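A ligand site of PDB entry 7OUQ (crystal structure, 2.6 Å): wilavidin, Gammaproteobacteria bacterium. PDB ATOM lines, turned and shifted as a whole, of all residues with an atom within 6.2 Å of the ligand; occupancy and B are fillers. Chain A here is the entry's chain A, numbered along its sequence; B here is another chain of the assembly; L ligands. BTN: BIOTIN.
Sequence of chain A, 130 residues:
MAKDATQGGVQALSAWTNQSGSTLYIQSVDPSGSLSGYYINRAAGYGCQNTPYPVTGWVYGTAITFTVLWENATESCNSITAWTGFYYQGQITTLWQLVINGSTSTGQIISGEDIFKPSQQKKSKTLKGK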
ATOM      1  N   ASN A  18      -7.073  17.352  23.073  1.00  0.00           N
ATOM      2  CA  ASN A  18      -8.494  17.633  23.403  1.00  0.00           C
ATOM      3  C   ASN A  18      -9.305  16.330  23.309  1.00  0.00           C
ATOM      4  O   ASN A  18      -8.744  15.283  22.972  1.00  0.00           O
ATOM      5  CB  ASN A  18      -9.062  18.791  22.563  1.00  0.00           C
ATOM      6  CG  ASN A  18      -9.236  18.479  21.086  1.00  0.00           C
ATOM      7  OD1 ASN A  18      -9.367  17.310  20.703  1.00  0.00           O
ATOM      8  ND2 ASN A  18      -9.242  19.519  20.260  1.00  0.00           N
ATOM      9  N   GLN A  19     -10.595  16.424  23.603  1.00  0.00           N
ATOM     10  CA  GLN A  19     -11.514  15.250  23.712  1.00  0.00           C
ATOM     11  C   GLN A  19     -11.860  14.718  22.315  1.00  0.00           C
ATOM     12  O   GLN A  19     -12.161  13.539  22.236  1.00  0.00           O
ATOM     13  CB  GLN A  19     -12.733  15.629  24.550  1.00  0.00           C
ATOM     14  CG  GLN A  19     -13.645  16.640  23.878  1.00  0.00           C
ATOM     15  CD  GLN A  19     -12.977  17.991  23.703  1.00  0.00           C
ATOM     16  OE1 GLN A  19     -12.573  18.609  24.700  1.00  0.00           O
ATOM     17  NE2 GLN A  19     -12.850  18.395  22.431  1.00  0.00           N
ATOM     18  N   SER A  20     -11.770  15.502  21.233  1.00  0.00           N
ATOM     19  CA  SER A  20     -11.942  15.018  19.828  1.00  0.00           C
ATOM     20  C   SER A  20     -10.669  14.261  19.372  1.00  0.00           C
ATOM     21  O   SER A  20     -10.715  13.682  18.251  1.00  0.00           O
ATOM     22  CB  SER A  20     -12.301  16.155  18.864  1.00  0.00           C
ATOM     23  OG  SER A  20     -12.975  17.229  19.525  1.00  0.00           O
ATOM     24  N   GLY A  21      -9.596  14.280  20.176  1.00  0.00           N
ATOM     25  CA  GLY A  21      -8.348  13.505  20.007  1.00  0.00           C
ATOM     26  C   GLY A  21      -7.225  14.286  19.331  1.00  0.00           C
ATOM     27  O   GLY A  21      -6.133  13.694  19.125  1.00  0.00           O
ATOM     28  N   SER A  22      -7.492  15.539  18.936  1.00  0.00           N
ATOM     29  CA  SER A  22      -6.534  16.507  18.360  1.00  0.00           C
ATOM     30  C   SER A  22      -5.474  16.870  19.401  1.00  0.00           C
ATOM     31  O   SER A  22      -5.773  16.737  20.594  1.00  0.00           O
ATOM     32  CB  SER A  22      -7.252  17.756  17.913  1.00  0.00           C
ATOM     33  OG  SER A  22      -8.212  17.503  16.895  1.00  0.00           O
ATOM     34  N   THR A  23      -4.304  17.352  18.958  1.00  0.00           N
ATOM     35  CA  THR A  23      -3.152  17.692  19.845  1.00  0.00           C
ATOM     36  C   THR A  23      -2.465  18.998  19.451  1.00  0.00           C
ATOM     37  O   THR A  23      -2.203  19.204  18.244  1.00  0.00           O
ATOM     38  CB  THR A  23      -2.068  16.615  19.843  1.00  0.00           C
ATOM     39  OG1 THR A  23      -2.669  15.402  20.267  1.00  0.00           O
ATOM     40  CG2 THR A  23      -0.923  16.980  20.748  1.00  0.00           C
ATOM     41  N   TYR A  39      -0.409  22.143  15.308  1.00  0.00           N
ATOM     42  CA  TYR A  39      -1.673  21.427  15.627  1.00  0.00           C
ATOM     43  C   TYR A  39      -1.745  20.218  14.703  1.00  0.00           C
ATOM     44  O   TYR A  39      -1.458  20.410  13.541  1.00  0.00           O
ATOM     45  CB  TYR A  39      -2.850  22.396  15.478  1.00  0.00           C
ATOM     46  CG  TYR A  39      -4.056  22.023  16.293  1.00  0.00           C
ATOM     47  CD1 TYR A  39      -4.187  22.457  17.593  1.00  0.00           C
ATOM     48  CD2 TYR A  39      -5.074  21.255  15.777  1.00  0.00           C
ATOM     49  CE1 TYR A  39      -5.304  22.180  18.348  1.00  0.00           C
ATOM     50  CE2 TYR A  39      -6.201  20.942  16.528  1.00  0.00           C
ATOM     51  CZ  TYR A  39      -6.320  21.407  17.823  1.00  0.00           C
ATOM     52  OH  TYR A  39      -7.415  21.124  18.577  1.00  0.00           O
ATOM     53  N   ILE A  40      -2.061  19.042  15.221  1.00  0.00           N
ATOM     54  CA  ILE A  40      -2.586  17.912  14.417  1.00  0.00           C
ATOM     55  C   ILE A  40      -4.076  17.735  14.778  1.00  0.00           C
ATOM     56  O   ILE A  40      -4.363  17.372  15.934  1.00  0.00           O
ATOM     57  CB  ILE A  40      -1.780  16.629  14.689  1.00  0.00           C
ATOM     58  CG1 ILE A  40      -0.332  16.745  14.213  1.00  0.00           C
ATOM     59  CG2 ILE A  40      -2.449  15.428  14.061  1.00  0.00           C
ATOM     60  CD1 ILE A  40       0.491  15.518  14.581  1.00  0.00           C
ATOM     61  N   ASN A  41      -4.983  17.926  13.796  1.00  0.00           N
ATOM     62  CA  ASN A  41      -6.458  17.774  13.952  1.00  0.00           C
ATOM     63  C   ASN A  41      -6.843  16.305  13.779  1.00  0.00           C
ATOM     64  O   ASN A  41      -6.491  15.731  12.766  1.00  0.00           O
ATOM     65  CB  ASN A  41      -7.176  18.682  12.939  1.00  0.00           C
ATOM     66  CG  ASN A  41      -8.667  18.444  12.855  1.00  0.00           C
ATOM     67  OD1 ASN A  41      -9.277  17.981  13.819  1.00  0.00           O
ATOM     68  ND2 ASN A  41      -9.260  18.854  11.731  1.00  0.00           N
ATOM     69  N   ARG A  42      -7.515  15.695  14.735  1.00  0.00           N
ATOM     70  CA  ARG A  42      -7.970  14.287  14.633  1.00  0.00           C
ATOM     71  C   ARG A  42      -9.482  14.210  14.914  1.00  0.00           C
ATOM     72  O   ARG A  42      -9.983  13.160  15.387  1.00  0.00           O
ATOM     73  CB  ARG A  42      -7.139  13.445  15.602  1.00  0.00           C
ATOM     74  CG  ARG A  42      -5.739  13.081  15.131  1.00  0.00           C
ATOM     75  CD  ARG A  42      -5.039  12.130  16.104  1.00  0.00           C
ATOM     76  NE  ARG A  42      -3.594  12.373  16.141  1.00  0.00           N
ATOM     77  CZ  ARG A  42      -2.977  13.280  16.896  1.00  0.00           C
ATOM     78  NH1 ARG A  42      -3.649  14.065  17.714  1.00  0.00           N
ATOM     79  NH2 ARG A  42      -1.666  13.416  16.805  1.00  0.00           N
ATOM     80  N   ALA A  43     -10.220  15.292  14.656  1.00  0.00           N
ATOM     81  CA  ALA A  43     -11.645  15.451  15.021  1.00  0.00           C
ATOM     82  C   ALA A  43     -12.541  14.909  13.912  1.00  0.00           C
ATOM     83  O   ALA A  43     -12.538  15.475  12.773  1.00  0.00           O
ATOM     84  CB  ALA A  43     -11.946  16.910  15.251  1.00  0.00           C
ATOM     85  N   GLY A  45     -15.253  14.385  11.395  1.00  0.00           N
ATOM     86  CA  GLY A  45     -16.126  15.227  10.564  1.00  0.00           C
ATOM     87  C   GLY A  45     -15.369  16.336   9.900  1.00  0.00           C
ATOM     88  O   GLY A  45     -15.990  17.029   9.104  1.00  0.00           O
ATOM     89  N   TYR A  46     -14.082  16.558  10.150  1.00  0.00           N
ATOM     90  CA  TYR A  46     -13.447  17.771   9.585  1.00  0.00           C
ATOM     91  C   TYR A  46     -12.438  17.449   8.485  1.00  0.00           C
ATOM     92  O   TYR A  46     -11.768  16.395   8.529  1.00  0.00           O
ATOM     93  CB  TYR A  46     -12.797  18.592  10.697  1.00  0.00           C
ATOM     94  CG  TYR A  46     -13.762  19.141  11.715  1.00  0.00           C
ATOM     95  CD1 TYR A  46     -14.199  18.343  12.753  1.00  0.00           C
ATOM     96  CD2 TYR A  46     -14.203  20.454  11.637  1.00  0.00           C
ATOM     97  CE1 TYR A  46     -15.065  18.852  13.708  1.00  0.00           C
ATOM     98  CE2 TYR A  46     -15.065  20.979  12.581  1.00  0.00           C
ATOM     99  CZ  TYR A  46     -15.492  20.167  13.620  1.00  0.00           C
ATOM    100  OH  TYR A  46     -16.318  20.671  14.582  1.00  0.00           O
ATOM    101  N   GLY A  47     -12.259  18.427   7.594  1.00  0.00           N
ATOM    102  CA  GLY A  47     -11.024  18.594   6.808  1.00  0.00           C
ATOM    103  C   GLY A  47      -9.751  18.526   7.648  1.00  0.00           C
ATOM    104  O   GLY A  47      -9.799  18.581   8.916  1.00  0.00           O
ATOM    105  N   CYS A  48      -8.615  18.378   6.974  1.00  0.00           N
ATOM    106  CA  CYS A  48      -7.269  18.741   7.493  1.00  0.00           C
ATOM    107  C   CYS A  48      -6.958  17.912   8.759  1.00  0.00           C
ATOM    108  O   CYS A  48      -6.462  18.471   9.794  1.00  0.00           O
ATOM    109  CB  CYS A  48      -7.191  20.257   7.658  1.00  0.00           C
ATOM    110  SG  CYS A  48      -7.302  21.204   6.100  1.00  0.00           S
ATOM    111  N   TRP A  70      -5.313  26.616   8.288  1.00  0.00           N
ATOM    112  CA  TRP A  70      -5.543  25.242   7.770  1.00  0.00           C
ATOM    113  C   TRP A  70      -5.069  25.227   6.312  1.00  0.00           C
ATOM    114  O   TRP A  70      -5.865  25.430   5.376  1.00  0.00           O
ATOM    115  CB  TRP A  70      -6.985  24.779   7.943  1.00  0.00           C
ATOM    116  CG  TRP A  70      -7.423  24.883   9.364  1.00  0.00           C
ATOM    117  CD1 TRP A  70      -8.189  25.860   9.931  1.00  0.00           C
ATOM    118  CD2 TRP A  70      -7.061  23.990  10.412  1.00  0.00           C
ATOM    119  NE1 TRP A  70      -8.381  25.592  11.260  1.00  0.00           N
ATOM    120  CE2 TRP A  70      -7.698  24.452  11.577  1.00  0.00           C
ATOM    121  CE3 TRP A  70      -6.327  22.810  10.454  1.00  0.00           C
ATOM    122  CZ2 TRP A  70      -7.589  23.794  12.785  1.00  0.00           C
ATOM    123  CZ3 TRP A  70      -6.226  22.138  11.656  1.00  0.00           C
ATOM    124  CH2 TRP A  70      -6.845  22.634  12.804  1.00  0.00           C
ATOM    125  N   CYS A  77      -8.003  23.756   3.850  1.00  0.00           N
ATOM    126  CA  CYS A  77      -9.459  23.765   4.155  1.00  0.00           C
ATOM    127  C   CYS A  77     -10.020  25.184   4.084  1.00  0.00           C
ATOM    128  O   CYS A  77     -11.165  25.382   4.448  1.00  0.00           O
ATOM    129  CB  CYS A  77      -9.751  23.133   5.516  1.00  0.00           C
ATOM    130  SG  CYS A  77      -9.378  21.349   5.623  1.00  0.00           S
ATOM    131  N   ASN A  78      -9.267  26.127   3.538  1.00  0.00           N
ATOM    132  CA  ASN A  78      -9.762  27.501   3.266  1.00  0.00           C
ATOM    133  C   ASN A  78     -10.386  28.158   4.516  1.00  0.00           C
ATOM    134  O   ASN A  78     -11.301  29.003   4.349  1.00  0.00           O
ATOM    135  CB  ASN A  78     -10.728  27.484   2.102  1.00  0.00           C
ATOM    136  CG  ASN A  78     -10.441  28.647   1.184  1.00  0.00           C
ATOM    137  OD1 ASN A  78      -9.329  28.773   0.689  1.00  0.00           O
ATOM    138  ND2 ASN A  78     -11.441  29.490   0.960  1.00  0.00           N
ATOM    139  N   SER A  79      -9.813  27.895   5.694  1.00  0.00           N
ATOM    140  CA  SER A  79     -10.314  28.382   7.009  1.00  0.00           C
ATOM    141  C   SER A  79      -9.175  28.664   8.010  1.00  0.00           C
ATOM    142  O   SER A  79      -8.076  28.111   7.870  1.00  0.00           O
ATOM    143  CB  SER A  79     -11.249  27.327   7.553  1.00  0.00           C
ATOM    144  OG  SER A  79     -10.578  26.085   7.759  1.00  0.00           O
ATOM    145  N   THR A  81      -9.006  28.693  12.508  1.00  0.00           N
ATOM    146  CA  THR A  81      -9.591  28.548  13.859  1.00  0.00           C
ATOM    147  C   THR A  81      -8.786  29.382  14.878  1.00  0.00           C
ATOM    148  O   THR A  81      -7.589  29.311  14.854  1.00  0.00           O
ATOM    149  CB  THR A  81      -9.586  27.086  14.317  1.00  0.00           C
ATOM    150  OG1 THR A  81     -10.341  26.269  13.420  1.00  0.00           O
ATOM    151  CG2 THR A  81     -10.090  26.940  15.737  1.00  0.00           C
ATOM    152  N   TRP A  83      -8.588  29.591  19.078  1.00  0.00           N
ATOM    153  CA  TRP A  83      -8.989  29.208  20.449  1.00  0.00           C
ATOM    154  C   TRP A  83      -8.649  30.337  21.429  1.00  0.00           C
ATOM    155  O   TRP A  83      -7.766  31.098  21.127  1.00  0.00           O
ATOM    156  CB  TRP A  83      -8.273  27.940  20.844  1.00  0.00           C
ATOM    157  CG  TRP A  83      -8.654  26.698  20.110  1.00  0.00           C
ATOM    158  CD1 TRP A  83      -9.343  25.636  20.624  1.00  0.00           C
ATOM    159  CD2 TRP A  83      -8.193  26.284  18.817  1.00  0.00           C
ATOM    160  NE1 TRP A  83      -9.337  24.596  19.750  1.00  0.00           N
ATOM    161  CE2 TRP A  83      -8.658  24.970  18.631  1.00  0.00           C
ATOM    162  CE3 TRP A  83      -7.423  26.885  17.828  1.00  0.00           C
ATOM    163  CZ2 TRP A  83      -8.382  24.244  17.480  1.00  0.00           C
ATOM    164  CZ3 TRP A  83      -7.141  26.178  16.691  1.00  0.00           C
ATOM    165  CH2 TRP A  83      -7.612  24.876  16.520  1.00  0.00           C
ATOM    166  N   TRP A  96     -13.504  28.080  20.940  1.00  0.00           N
ATOM    167  CA  TRP A  96     -12.956  28.351  19.602  1.00  0.00           C
ATOM    168  C   TRP A  96     -14.022  28.945  18.682  1.00  0.00           C
ATOM    169  O   TRP A  96     -15.207  28.782  18.917  1.00  0.00           O
ATOM    170  CB  TRP A  96     -12.298  27.080  19.062  1.00  0.00           C
ATOM    171  CG  TRP A  96     -13.167  25.884  18.845  1.00  0.00           C
ATOM    172  CD1 TRP A  96     -13.203  24.728  19.584  1.00  0.00           C
ATOM    173  CD2 TRP A  96     -14.034  25.664  17.723  1.00  0.00           C
ATOM    174  NE1 TRP A  96     -14.052  23.822  19.011  1.00  0.00           N
ATOM    175  CE2 TRP A  96     -14.559  24.350  17.861  1.00  0.00           C
ATOM    176  CE3 TRP A  96     -14.406  26.438  16.615  1.00  0.00           C
ATOM    177  CZ2 TRP A  96     -15.425  23.800  16.924  1.00  0.00           C
ATOM    178  CZ3 TRP A  96     -15.280  25.904  15.701  1.00  0.00           C
ATOM    179  CH2 TRP A  96     -15.780  24.596  15.858  1.00  0.00           C
ATOM    180  N   LEU A  98     -14.255  29.693  14.285  1.00  0.00           N
ATOM    181  CA  LEU A  98     -13.684  29.189  13.009  1.00  0.00           C
ATOM    182  C   LEU A  98     -14.302  29.995  11.875  1.00  0.00           C
ATOM    183  O   LEU A  98     -15.521  30.050  11.787  1.00  0.00           O
ATOM    184  CB  LEU A  98     -13.961  27.685  12.863  1.00  0.00           C
ATOM    185  CG  LEU A  98     -13.281  27.022  11.664  1.00  0.00           C
ATOM    186  CD1 LEU A  98     -13.275  25.494  11.784  1.00  0.00           C
ATOM    187  CD2 LEU A  98     -13.944  27.469  10.359  1.00  0.00           C
ATOM    188  N   ILE A 100     -14.413  30.798   7.691  1.00  0.00           N
ATOM    189  CA  ILE A 100     -14.125  30.205   6.371  1.00  0.00           C
ATOM    190  C   ILE A 100     -13.823  31.370   5.444  1.00  0.00           C
ATOM    191  O   ILE A 100     -14.554  32.383   5.445  1.00  0.00           O
ATOM    192  CB  ILE A 100     -15.298  29.335   5.921  1.00  0.00           C
ATOM    193  CG1 ILE A 100     -15.403  28.080   6.781  1.00  0.00           C
ATOM    194  CG2 ILE A 100     -15.190  29.007   4.433  1.00  0.00           C
ATOM    195  CD1 ILE A 100     -16.793  27.506   6.873  1.00  0.00           C
ATOM    196  N   ASP A 114     -13.174  23.155  23.349  1.00  0.00           N
ATOM    197  CA  ASP A 114     -12.138  22.109  23.474  1.00  0.00           C
ATOM    198  C   ASP A 114     -11.557  22.218  24.865  1.00  0.00           C
ATOM    199  O   ASP A 114     -11.374  23.348  25.360  1.00  0.00           O
ATOM    200  CB  ASP A 114     -11.054  22.225  22.411  1.00  0.00           C
ATOM    201  CG  ASP A 114     -11.462  21.734  21.037  1.00  0.00           C
ATOM    202  OD1 ASP A 114     -12.087  20.625  20.940  1.00  0.00           O
ATOM    203  OD2 ASP A 114     -11.152  22.445  20.079  1.00  0.00           O
ATOM    204  N   PHE A 116      -8.239  20.551  26.620  1.00  0.00           N
ATOM    205  CA  PHE A 116      -6.945  19.872  26.335  1.00  0.00           C
ATOM    206  C   PHE A 116      -6.308  19.415  27.651  1.00  0.00           C
ATOM    207  O   PHE A 116      -6.116  20.217  28.589  1.00  0.00           O
ATOM    208  CB  PHE A 116      -6.008  20.799  25.587  1.00  0.00           C
ATOM    209  CG  PHE A 116      -6.489  21.305  24.257  1.00  0.00           C
ATOM    210  CD1 PHE A 116      -7.219  22.470  24.174  1.00  0.00           C
ATOM    211  CD2 PHE A 116      -6.136  20.662  23.075  1.00  0.00           C
ATOM    212  CE1 PHE A 116      -7.644  22.968  22.949  1.00  0.00           C
ATOM    213  CE2 PHE A 116      -6.550  21.167  21.848  1.00  0.00           C
ATOM    214  CZ  PHE A 116      -7.299  22.327  21.788  1.00  0.00           C
ATOM    215  N   LYS B 125     -13.048  20.611   3.309  1.00  0.00           N
ATOM    216  CA  LYS B 125     -14.160  21.172   4.095  1.00  0.00           C
ATOM    217  C   LYS B 125     -15.461  20.755   3.374  1.00  0.00           C
ATOM    218  O   LYS B 125     -15.738  20.888   2.144  1.00  0.00           O
ATOM    219  CB  LYS B 125     -13.958  22.693   4.355  1.00  0.00           C
ATOM    220  CG  LYS B 125     -14.531  23.333   5.637  1.00  0.00           C
ATOM    221  CD  LYS B 125     -14.673  22.421   6.880  1.00  0.00           C
ATOM    222  CE  LYS B 125     -15.259  21.023   6.645  1.00  0.00           C
ATOM    223  NZ  LYS B 125     -15.717  20.419   7.909  1.00  0.00           N
HETATM  224  C11 BTN L   1     -11.525  22.504   8.669  1.00  0.00           C
HETATM  225  O11 BTN L   1     -12.426  21.632   8.709  1.00  0.00           O
HETATM  226  O12 BTN L   1     -11.643  23.664   8.165  1.00  0.00           O
HETATM  227  C10 BTN L   1     -10.207  22.018   9.245  1.00  0.00           C
HETATM  228  C9  BTN L   1      -9.968  22.516  10.640  1.00  0.00           C
HETATM  229  C8  BTN L   1     -11.059  22.189  11.633  1.00  0.00           C
HETATM  230  C7  BTN L   1     -10.584  21.458  12.890  1.00  0.00           C
HETATM  231  C2  BTN L   1     -11.423  22.000  14.025  1.00  0.00           C
HETATM  232  S1  BTN L   1     -10.767  23.465  14.664  1.00  0.00           S
HETATM  233  C6  BTN L   1     -11.672  23.353  16.153  1.00  0.00           C
HETATM  234  C5  BTN L   1     -11.992  21.911  16.397  1.00  0.00           C
HETATM  235  N1  BTN L   1     -11.117  21.374  17.371  1.00  0.00           N
HETATM  236  C3  BTN L   1     -10.304  20.438  16.908  1.00  0.00           C
HETATM  237  O3  BTN L   1      -9.578  19.736  17.596  1.00  0.00           O
HETATM  238  N2  BTN L   1     -10.503  20.329  15.611  1.00  0.00           N
HETATM  239  C4  BTN L   1     -11.639  21.079  15.184  1.00  0.00           C
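OG of Ser 79 sits at hydrogen-bond distance from O12 of the ligand, at 2.7 Å. The side-chain amide nitrogen (ND2) of Asn 18 sits at hydrogen-bond distance from an oxygen (O3) of the ligand (2.7 Å). O3 of the ligand lies within hydrogen-bond range of OG of Ser 22, at 2.7 Å. An oxygen (O3) of the ligand sits at hydrogen-bond distance from the side-chain hydroxyl of Tyr 39, 2.8 Å away. The side-chain carboxylate of Asp 114 is in hydrogen-bond range of a nitrogen (N1) of the ligand, at 2.9 Å. NZ of Lys 125 of chain B lies within salt-bridge range of O11 of the ligand, 3.6 Å away. The side-chain hydroxyl (OG1) of Thr 81 sits close to a sulfur (S1) of the ligand (3.1 Å). The side-chain amide oxygen (OD1) of Asn 41 is in hydrogen-bond range of a nitrogen (N2) of the ligand (3.2 Å). The backbone NH (N) of Gly 47 lies within hydrogen-bond range of an oxygen (O11) of the ligand (3.4 Å).
The side-chain hydroxyl (OG) of Ser 79 lies within hydrogen-bond range of the backbone carbonyl oxygen (O) of Cys 77 (3.4 Å). OD1 of Asn 18 is in hydrogen-bond range of N of Ser 22 (3.1 Å). The side-chain carboxylate of Asp 114 lies within hydrogen-bond range of the side-chain amide nitrogen of Asn 18, 3.1 Å away. The backbone NH (N) of Ser 20 is in hydrogen-bond range of the side-chain amide oxygen (OD1) of Asn 18 (3.1 Å). The side-chain amide oxygen (OD1) of Asn 41 sits at hydrogen-bond distance from the side-chain hydroxyl (OG) of Ser 22 (3.3 Å). N of Arg 42 sits at hydrogen-bond distance from OG of Ser 22, 2.9 Å away. The side-chain amide nitrogen (ND2) of Asn 41 lies within hydrogen-bond range of the backbone carbonyl oxygen (O) of Gly 47. The backbone carbonyl oxygen (O) of Cys 48 lies close to the side-chain amide nitrogen (ND2) of Asn 41 (3.4 Å).
CB of Ala 43 touches N2 of the ligand, at 3.7 Å. Tyr 46 touches the ligand (CD2 to C8, 3.6 Å). Cys 48 touches the ligand. CE2 of Trp 70 touches C9 of the ligand (3.1 Å). Cys 77 touches the ligand. Trp 83 touches the ligand (CZ2 to C6, 3.7 Å). Trp 96 touches the ligand (CE2 to C6, 3.5 Å). CD1 of Leu 98 touches C8 of the ligand, at 3.98 Å. Of the 27 residues printed, 17 come within 4 Å of the ligand.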
